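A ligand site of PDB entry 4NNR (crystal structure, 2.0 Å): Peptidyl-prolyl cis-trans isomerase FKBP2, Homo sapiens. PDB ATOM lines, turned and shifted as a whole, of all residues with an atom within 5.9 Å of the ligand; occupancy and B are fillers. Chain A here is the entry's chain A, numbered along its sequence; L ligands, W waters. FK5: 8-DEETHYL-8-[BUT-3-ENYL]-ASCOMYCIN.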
ATOM      1  N   TYR A  56     -16.070  28.774  -4.733  1.00  0.00           N
ATOM      2  CA  TYR A  56     -14.763  28.244  -4.385  1.00  0.00           C
ATOM      3  C   TYR A  56     -13.637  28.762  -5.230  1.00  0.00           C
ATOM      4  O   TYR A  56     -13.824  29.249  -6.336  1.00  0.00           O
ATOM      5  CB  TYR A  56     -14.787  26.702  -4.458  1.00  0.00           C
ATOM      6  CG  TYR A  56     -14.831  26.177  -5.854  1.00  0.00           C
ATOM      7  CD1 TYR A  56     -13.673  25.882  -6.521  1.00  0.00           C
ATOM      8  CD2 TYR A  56     -16.040  25.999  -6.527  1.00  0.00           C
ATOM      9  CE1 TYR A  56     -13.685  25.410  -7.789  1.00  0.00           C
ATOM     10  CE2 TYR A  56     -16.049  25.530  -7.825  1.00  0.00           C
ATOM     11  CZ  TYR A  56     -14.867  25.228  -8.443  1.00  0.00           C
ATOM     12  OH  TYR A  56     -14.819  24.755  -9.732  1.00  0.00           O
ATOM     13  N   GLY A  58      -9.752  27.073  -6.018  1.00  0.00           N
ATOM     14  CA  GLY A  58      -8.805  25.978  -5.817  1.00  0.00           C
ATOM     15  C   GLY A  58      -7.380  26.390  -6.204  1.00  0.00           C
ATOM     16  O   GLY A  58      -7.156  26.972  -7.250  1.00  0.00           O
ATOM     17  N   PHE A  66      -5.991  27.022  -9.865  1.00  0.00           N
ATOM     18  CA  PHE A  66      -6.384  26.173 -10.999  1.00  0.00           C
ATOM     19  C   PHE A  66      -7.872  26.254 -11.387  1.00  0.00           C
ATOM     20  O   PHE A  66      -8.243  25.802 -12.456  1.00  0.00           O
ATOM     21  CB  PHE A  66      -6.016  24.725 -10.744  1.00  0.00           C
ATOM     22  CG  PHE A  66      -6.758  24.069  -9.607  1.00  0.00           C
ATOM     23  CD1 PHE A  66      -6.135  23.865  -8.392  1.00  0.00           C
ATOM     24  CD2 PHE A  66      -8.053  23.579  -9.770  1.00  0.00           C
ATOM     25  CE1 PHE A  66      -6.794  23.228  -7.342  1.00  0.00           C
ATOM     26  CE2 PHE A  66      -8.731  22.947  -8.745  1.00  0.00           C
ATOM     27  CZ  PHE A  66      -8.104  22.761  -7.521  1.00  0.00           C
ATOM     28  N   ASP A  67      -8.695  26.829 -10.527  1.00  0.00           N
ATOM     29  CA  ASP A  67     -10.120  26.969 -10.810  1.00  0.00           C
ATOM     30  C   ASP A  67     -10.785  27.835  -9.777  1.00  0.00           C
ATOM     31  O   ASP A  67     -10.385  27.877  -8.618  1.00  0.00           O
ATOM     32  CB  ASP A  67     -10.825  25.611 -10.830  1.00  0.00           C
ATOM     33  CG  ASP A  67     -12.177  25.653 -11.541  1.00  0.00           C
ATOM     34  OD1 ASP A  67     -12.468  26.668 -12.220  1.00  0.00           O
ATOM     35  OD2 ASP A  67     -12.936  24.662 -11.453  1.00  0.00           O
ATOM     36  N   PHE A  76     -21.343  26.865  -7.499  1.00  0.00           N
ATOM     37  CA  PHE A  76     -21.354  25.432  -7.715  1.00  0.00           C
ATOM     38  C   PHE A  76     -22.421  24.844  -6.805  1.00  0.00           C
ATOM     39  O   PHE A  76     -22.529  25.231  -5.657  1.00  0.00           O
ATOM     40  CB  PHE A  76     -19.967  24.877  -7.437  1.00  0.00           C
ATOM     41  CG  PHE A  76     -19.877  23.380  -7.442  1.00  0.00           C
ATOM     42  CD1 PHE A  76     -19.721  22.687  -6.260  1.00  0.00           C
ATOM     43  CD2 PHE A  76     -19.904  22.676  -8.636  1.00  0.00           C
ATOM     44  CE1 PHE A  76     -19.639  21.318  -6.243  1.00  0.00           C
ATOM     45  CE2 PHE A  76     -19.800  21.302  -8.641  1.00  0.00           C
ATOM     46  CZ  PHE A  76     -19.676  20.603  -7.436  1.00  0.00           C
ATOM     47  N   GLN A  84     -20.837  12.880  -5.000  1.00  0.00           N
ATOM     48  CA  GLN A  84     -20.826  13.685  -6.215  1.00  0.00           C
ATOM     49  C   GLN A  84     -19.451  14.382  -6.406  1.00  0.00           C
ATOM     50  O   GLN A  84     -19.020  14.669  -7.536  1.00  0.00           O
ATOM     51  CB  GLN A  84     -21.979  14.703  -6.132  1.00  0.00           C
ATOM     52  CG  GLN A  84     -22.091  15.651  -7.291  1.00  0.00           C
ATOM     53  CD  GLN A  84     -23.349  16.493  -7.228  1.00  0.00           C
ATOM     54  OE1 GLN A  84     -24.159  16.357  -6.310  1.00  0.00           O
ATOM     55  NE2 GLN A  84     -23.535  17.364  -8.215  1.00  0.00           N
ATOM     56  N   VAL A  85     -18.767  14.599  -5.291  1.00  0.00           N
ATOM     57  CA  VAL A  85     -17.522  15.366  -5.264  1.00  0.00           C
ATOM     58  C   VAL A  85     -16.419  14.558  -4.579  1.00  0.00           C
ATOM     59  O   VAL A  85     -16.659  13.524  -3.952  1.00  0.00           O
ATOM     60  CB  VAL A  85     -17.693  16.736  -4.537  1.00  0.00           C
ATOM     61  CG1 VAL A  85     -18.520  17.687  -5.355  1.00  0.00           C
ATOM     62  CG2 VAL A  85     -18.276  16.564  -3.138  1.00  0.00           C
ATOM     63  N   ILE A  86     -15.195  15.024  -4.713  1.00  0.00           N
ATOM     64  CA  ILE A  86     -14.080  14.315  -4.089  1.00  0.00           C
ATOM     65  C   ILE A  86     -14.323  14.195  -2.585  1.00  0.00           C
ATOM     66  O   ILE A  86     -15.084  14.985  -1.999  1.00  0.00           O
ATOM     67  CB  ILE A  86     -12.763  15.037  -4.391  1.00  0.00           C
ATOM     68  CG1 ILE A  86     -12.815  16.513  -3.972  1.00  0.00           C
ATOM     69  CG2 ILE A  86     -12.493  14.967  -5.871  1.00  0.00           C
ATOM     70  CD1 ILE A  86     -11.506  17.274  -4.152  1.00  0.00           C
ATOM     71  N   LYS A  87     -13.695  13.207  -1.950  1.00  0.00           N
ATOM     72  CA  LYS A  87     -13.971  12.849  -0.571  1.00  0.00           C
ATOM     73  C   LYS A  87     -13.666  13.986   0.378  1.00  0.00           C
ATOM     74  O   LYS A  87     -14.372  14.161   1.365  1.00  0.00           O
ATOM     75  CB  LYS A  87     -13.164  11.617  -0.168  1.00  0.00           C
ATOM     76  CG  LYS A  87     -13.575  10.368  -0.911  1.00  0.00           C
ATOM     77  CD  LYS A  87     -14.609   9.524  -0.178  1.00  0.00           C
ATOM     78  CE  LYS A  87     -14.295   8.020  -0.273  1.00  0.00           C
ATOM     79  NZ  LYS A  87     -12.909   7.657   0.229  1.00  0.00           N
ATOM     80  N   TRP A  89     -14.078  17.092   0.024  1.00  0.00           N
ATOM     81  CA  TRP A  89     -15.212  18.004   0.105  1.00  0.00           C
ATOM     82  C   TRP A  89     -16.331  17.391   0.954  1.00  0.00           C
ATOM     83  O   TRP A  89     -16.803  18.022   1.883  1.00  0.00           O
ATOM     84  CB  TRP A  89     -15.721  18.363  -1.292  1.00  0.00           C
ATOM     85  CG  TRP A  89     -15.080  19.569  -1.871  1.00  0.00           C
ATOM     86  CD1 TRP A  89     -13.743  19.799  -2.012  1.00  0.00           C
ATOM     87  CD2 TRP A  89     -15.747  20.732  -2.410  1.00  0.00           C
ATOM     88  NE1 TRP A  89     -13.532  21.030  -2.611  1.00  0.00           N
ATOM     89  CE2 TRP A  89     -14.733  21.618  -2.847  1.00  0.00           C
ATOM     90  CE3 TRP A  89     -17.085  21.097  -2.566  1.00  0.00           C
ATOM     91  CZ2 TRP A  89     -15.044  22.857  -3.443  1.00  0.00           C
ATOM     92  CZ3 TRP A  89     -17.385  22.326  -3.148  1.00  0.00           C
ATOM     93  CH2 TRP A  89     -16.360  23.194  -3.576  1.00  0.00           C
ATOM     94  N   GLY A 111      -8.525  13.344  -2.794  1.00  0.00           N
ATOM     95  CA  GLY A 111      -8.697  14.189  -3.975  1.00  0.00           C
ATOM     96  C   GLY A 111      -8.654  13.334  -5.215  1.00  0.00           C
ATOM     97  O   GLY A 111      -9.493  12.461  -5.363  1.00  0.00           O
ATOM     98  N   TYR A 112      -7.656  13.515  -6.068  1.00  0.00           N
ATOM     99  CA  TYR A 112      -7.599  12.810  -7.335  1.00  0.00           C
ATOM    100  C   TYR A 112      -6.534  11.702  -7.390  1.00  0.00           C
ATOM    101  O   TYR A 112      -6.232  11.140  -8.453  1.00  0.00           O
ATOM    102  CB  TYR A 112      -7.387  13.827  -8.440  1.00  0.00           C
ATOM    103  CG  TYR A 112      -8.591  14.742  -8.578  1.00  0.00           C
ATOM    104  CD1 TYR A 112      -8.592  16.010  -8.022  1.00  0.00           C
ATOM    105  CD2 TYR A 112      -9.746  14.303  -9.210  1.00  0.00           C
ATOM    106  CE1 TYR A 112      -9.666  16.835  -8.124  1.00  0.00           C
ATOM    107  CE2 TYR A 112     -10.850  15.126  -9.319  1.00  0.00           C
ATOM    108  CZ  TYR A 112     -10.798  16.400  -8.774  1.00  0.00           C
ATOM    109  OH  TYR A 112     -11.893  17.239  -8.850  1.00  0.00           O
ATOM    110  N   ARG A 115      -3.512   9.471 -10.303  1.00  0.00           N
ATOM    111  CA  ARG A 115      -3.679   9.857 -11.703  1.00  0.00           C
ATOM    112  C   ARG A 115      -3.962  11.352 -11.862  1.00  0.00           C
ATOM    113  O   ARG A 115      -3.752  11.935 -12.926  1.00  0.00           O
ATOM    114  CB  ARG A 115      -4.787   9.043 -12.384  1.00  0.00           C
ATOM    115  CG  ARG A 115      -6.136   9.107 -11.731  1.00  0.00           C
ATOM    116  CD  ARG A 115      -7.229   8.779 -12.769  1.00  0.00           C
ATOM    117  NE  ARG A 115      -8.514   8.445 -12.149  1.00  0.00           N
ATOM    118  CZ  ARG A 115      -9.302   9.325 -11.507  1.00  0.00           C
ATOM    119  NH1 ARG A 115      -8.943  10.605 -11.366  1.00  0.00           N
ATOM    120  NH2 ARG A 115     -10.441   8.901 -10.985  1.00  0.00           N
ATOM    121  N   ALA A 117      -5.889  14.842 -12.386  1.00  0.00           N
ATOM    122  CA  ALA A 117      -6.983  15.334 -13.194  1.00  0.00           C
ATOM    123  C   ALA A 117      -6.372  16.242 -14.238  1.00  0.00           C
ATOM    124  O   ALA A 117      -6.525  17.482 -14.180  1.00  0.00           O
ATOM    125  CB  ALA A 117      -8.010  16.064 -12.335  1.00  0.00           C
ATOM    126  N   LYS A 120      -5.125  20.168 -15.205  1.00  0.00           N
ATOM    127  CA  LYS A 120      -5.000  21.182 -14.175  1.00  0.00           C
ATOM    128  C   LYS A 120      -4.425  20.631 -12.894  1.00  0.00           C
ATOM    129  O   LYS A 120      -3.891  21.396 -12.087  1.00  0.00           O
ATOM    130  CB  LYS A 120      -6.340  21.865 -13.870  1.00  0.00           C
ATOM    131  CG  LYS A 120      -7.572  21.131 -14.287  1.00  0.00           C
ATOM    132  CD  LYS A 120      -8.804  21.911 -13.857  1.00  0.00           C
ATOM    133  CE  LYS A 120      -8.958  23.205 -14.636  1.00  0.00           C
ATOM    134  NZ  LYS A 120     -10.208  23.913 -14.302  1.00  0.00           N
ATOM    135  N   ILE A 121      -4.521  19.332 -12.707  1.00  0.00           N
ATOM    136  CA  ILE A 121      -4.114  18.742 -11.444  1.00  0.00           C
ATOM    137  C   ILE A 121      -3.191  17.561 -11.697  1.00  0.00           C
ATOM    138  O   ILE A 121      -3.571  16.624 -12.369  1.00  0.00           O
ATOM    139  CB  ILE A 121      -5.339  18.325 -10.622  1.00  0.00           C
ATOM    140  CG1 ILE A 121      -6.115  19.587 -10.229  1.00  0.00           C
ATOM    141  CG2 ILE A 121      -4.915  17.550  -9.383  1.00  0.00           C
ATOM    142  CD1 ILE A 121      -7.393  19.318  -9.495  1.00  0.00           C
ATOM    143  N   LEU A 127      -4.398  19.717  -2.540  1.00  0.00           N
ATOM    144  CA  LEU A 127      -5.224  20.770  -3.052  1.00  0.00           C
ATOM    145  C   LEU A 127      -5.637  21.663  -1.902  1.00  0.00           C
ATOM    146  O   LEU A 127      -5.967  21.169  -0.809  1.00  0.00           O
ATOM    147  CB  LEU A 127      -6.445  20.181  -3.747  1.00  0.00           C
ATOM    148  CG  LEU A 127      -6.175  19.086  -4.768  1.00  0.00           C
ATOM    149  CD1 LEU A 127      -7.493  18.480  -5.289  1.00  0.00           C
ATOM    150  CD2 LEU A 127      -5.329  19.622  -5.913  1.00  0.00           C
ATOM    151  N   PHE A 129      -8.514  24.415  -1.081  1.00  0.00           N
ATOM    152  CA  PHE A 129      -9.737  25.105  -1.478  1.00  0.00           C
ATOM    153  C   PHE A 129     -10.161  26.115  -0.416  1.00  0.00           C
ATOM    154  O   PHE A 129     -10.218  25.793   0.774  1.00  0.00           O
ATOM    155  CB  PHE A 129     -10.891  24.128  -1.729  1.00  0.00           C
ATOM    156  CG  PHE A 129     -10.722  23.237  -2.923  1.00  0.00           C
ATOM    157  CD1 PHE A 129     -10.125  21.987  -2.800  1.00  0.00           C
ATOM    158  CD2 PHE A 129     -11.221  23.624  -4.160  1.00  0.00           C
ATOM    159  CE1 PHE A 129     -10.008  21.114  -3.923  1.00  0.00           C
ATOM    160  CE2 PHE A 129     -11.132  22.787  -5.278  1.00  0.00           C
ATOM    161  CZ  PHE A 129     -10.515  21.527  -5.164  1.00  0.00           C
HETATM  162  C1  FK5 L   1     -15.008  18.076  -7.646  1.00  0.00           C
HETATM  163  C2  FK5 L   1     -14.205  19.205  -7.081  1.00  0.00           C
HETATM  164  C3  FK5 L   1     -14.928  19.755  -5.863  1.00  0.00           C
HETATM  165  C4  FK5 L   1     -16.129  20.583  -6.227  1.00  0.00           C
HETATM  166  C5  FK5 L   1     -15.780  21.702  -7.184  1.00  0.00           C
HETATM  167  C6  FK5 L   1     -15.022  21.207  -8.409  1.00  0.00           C
HETATM  168  C8  FK5 L   1     -12.677  20.476  -8.471  1.00  0.00           C
HETATM  169  C9  FK5 L   1     -12.396  21.525  -9.315  1.00  0.00           C
HETATM  170  C10 FK5 L   1     -12.457  21.396 -10.823  1.00  0.00           C
HETATM  171  C11 FK5 L   1     -11.935  20.043 -11.300  1.00  0.00           C
HETATM  172  C12 FK5 L   1     -12.289  19.881 -12.790  1.00  0.00           C
HETATM  173  C13 FK5 L   1     -13.771  20.114 -12.990  1.00  0.00           C
HETATM  174  C14 FK5 L   1     -14.089  21.543 -12.557  1.00  0.00           C
HETATM  175  C15 FK5 L   1     -15.527  22.012 -12.808  1.00  0.00           C
HETATM  176  C16 FK5 L   1     -16.643  21.037 -12.362  1.00  0.00           C
HETATM  177  C17 FK5 L   1     -18.040  21.645 -12.521  1.00  0.00           C
HETATM  178  C18 FK5 L   1     -18.629  21.403 -13.926  1.00  0.00           C
HETATM  179  C19 FK5 L   1     -19.134  19.970 -14.050  1.00  0.00           C
HETATM  180  C20 FK5 L   1     -18.277  18.959 -14.664  1.00  0.00           C
HETATM  181  C21 FK5 L   1     -18.574  17.488 -14.664  1.00  0.00           C
HETATM  182  C22 FK5 L   1     -18.084  16.919 -13.383  1.00  0.00           C
HETATM  183  C23 FK5 L   1     -18.960  16.740 -12.187  1.00  0.00           C
HETATM  184  C24 FK5 L   1     -18.096  16.343 -10.999  1.00  0.00           C
HETATM  185  C25 FK5 L   1     -17.147  17.442 -10.430  1.00  0.00           C
HETATM  186  C26 FK5 L   1     -16.256  16.968  -9.259  1.00  0.00           C
HETATM  187  C27 FK5 L   1     -15.393  15.858  -9.753  1.00  0.00           C
HETATM  188  C28 FK5 L   1     -15.537  14.529  -9.190  1.00  0.00           C
HETATM  189  C29 FK5 L   1     -14.765  13.361  -9.738  1.00  0.00           C
HETATM  190  C30 FK5 L   1     -14.018  12.670  -8.581  1.00  0.00           C
HETATM  191  C31 FK5 L   1     -13.336  11.406  -9.089  1.00  0.00           C
HETATM  192  C32 FK5 L   1     -14.445  10.460  -9.564  1.00  0.00           C
HETATM  193  C33 FK5 L   1     -15.160  11.087 -10.762  1.00  0.00           C
HETATM  194  C34 FK5 L   1     -15.765  12.443 -10.434  1.00  0.00           C
HETATM  195  C35 FK5 L   1     -10.449  19.868 -11.079  1.00  0.00           C
HETATM  196  C36 FK5 L   1     -18.014  23.143 -12.213  1.00  0.00           C
HETATM  197  C37 FK5 L   1     -20.496  19.647 -13.551  1.00  0.00           C
HETATM  198  C38 FK5 L   1     -17.754  16.774 -15.738  1.00  0.00           C
HETATM  199  C39 FK5 L   1     -18.296  17.059 -17.113  1.00  0.00           C
HETATM  200  C40 FK5 L   1     -18.992  15.995 -17.842  1.00  0.00           C
HETATM  201  C41 FK5 L   1     -17.850  18.720  -9.983  1.00  0.00           C
HETATM  202  C42 FK5 L   1     -14.409  16.131 -10.842  1.00  0.00           C
HETATM  203  C43 FK5 L   1     -13.942  18.473 -14.595  1.00  0.00           C
HETATM  204  C44 FK5 L   1     -15.294  23.629 -14.507  1.00  0.00           C
HETATM  205  C45 FK5 L   1     -13.128  10.621  -6.887  1.00  0.00           C
HETATM  206  N7  FK5 L   1     -13.928  20.297  -8.025  1.00  0.00           N
HETATM  207  O1  FK5 L   1     -15.413  18.034  -8.846  1.00  0.00           O
HETATM  208  O2  FK5 L   1     -15.294  17.045  -6.770  1.00  0.00           O
HETATM  209  O3  FK5 L   1     -11.610  19.670  -8.080  1.00  0.00           O
HETATM  210  O4  FK5 L   1     -12.084  22.732  -8.739  1.00  0.00           O
HETATM  211  O5  FK5 L   1     -13.828  21.585 -11.176  1.00  0.00           O
HETATM  212  O6  FK5 L   1     -11.667  22.446 -11.443  1.00  0.00           O
HETATM  213  O7  FK5 L   1     -14.130  19.848 -14.325  1.00  0.00           O
HETATM  214  O8  FK5 L   1     -15.673  22.311 -14.183  1.00  0.00           O
HETATM  215  O9  FK5 L   1     -16.741  16.522 -13.298  1.00  0.00           O
HETATM  216  O10 FK5 L   1     -19.081  15.984 -10.072  1.00  0.00           O
HETATM  217  O11 FK5 L   1     -12.464  10.881  -8.115  1.00  0.00           O
HETATM  218  O12 FK5 L   1     -13.967   9.198  -9.957  1.00  0.00           O
HETATM  219  O   HOH W   1     -21.473  17.117 -10.403  1.00  0.00           O
HETATM  220  O   HOH W   2     -12.565  25.600 -15.255  1.00  0.00           O
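The side-chain carboxylate (OD2) of Asp 67 sits at hydrogen-bond distance from an oxygen (O6) of the ligand (2.6 Å). An oxygen (O3) of the ligand lies within hydrogen-bond range of the side-chain hydroxyl of Tyr 112. O10 of the ligand sits at hydrogen-bond distance from O of Gln 84 (2.9 Å). N of Ile 86 sits at hydrogen-bond distance from O2 of the ligand.
OD2 of Asp 67 is in hydrogen-bond range of OH of Tyr 56 (2.6 Å). The backbone carbonyl oxygen of Asp 67 is in hydrogen-bond range of the backbone NH of Gly 58 (2.8 Å). O of Phe 66 is in hydrogen-bond range of NZ of Lys 120 (3.3 Å). The backbone NH of Phe 66 sits at hydrogen-bond distance from the backbone carbonyl oxygen of Gly 58.
Tyr 56 touches the ligand (CE1 to O4, 3.3 Å). CE2 of Phe 66 touches O4 of the ligand, 3.4 Å away. Phe 76 touches the ligand (CE2 to C41, 3.5 Å). Val 85 touches the ligand (CA to O2, 3.2 Å). Trp 89 touches the ligand. NH2 of Arg 115 touches O12 of the ligand, at 3.7 Å. Lys 120 touches the ligand (NZ to O6, 3.5 Å). Ile 121 touches the ligand (CD1 to C35, 3.5 Å). Phe 129 touches the ligand (CE2 to O4, 3.6 Å). 13 residues have an atom within 4 Å of the ligand: Tyr 56, Phe 66, Asp 67, Phe 76, Gln 84, Val 85, Ile 86, Trp 89, Tyr 112, Arg 115, Lys 120, Ile 121 and Phe 129. The nearest printed residue that does not touch the ligand is Gly 111 (4.3 Å).
Water W1 lies within hydrogen-bond range of O10 of the ligand (2.7 Å) and NE2 of Gln 84 (3.0 Å). Water W2 lies within hydrogen-bond range of NZ of Lys 120 and OD1 of Asp 67.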
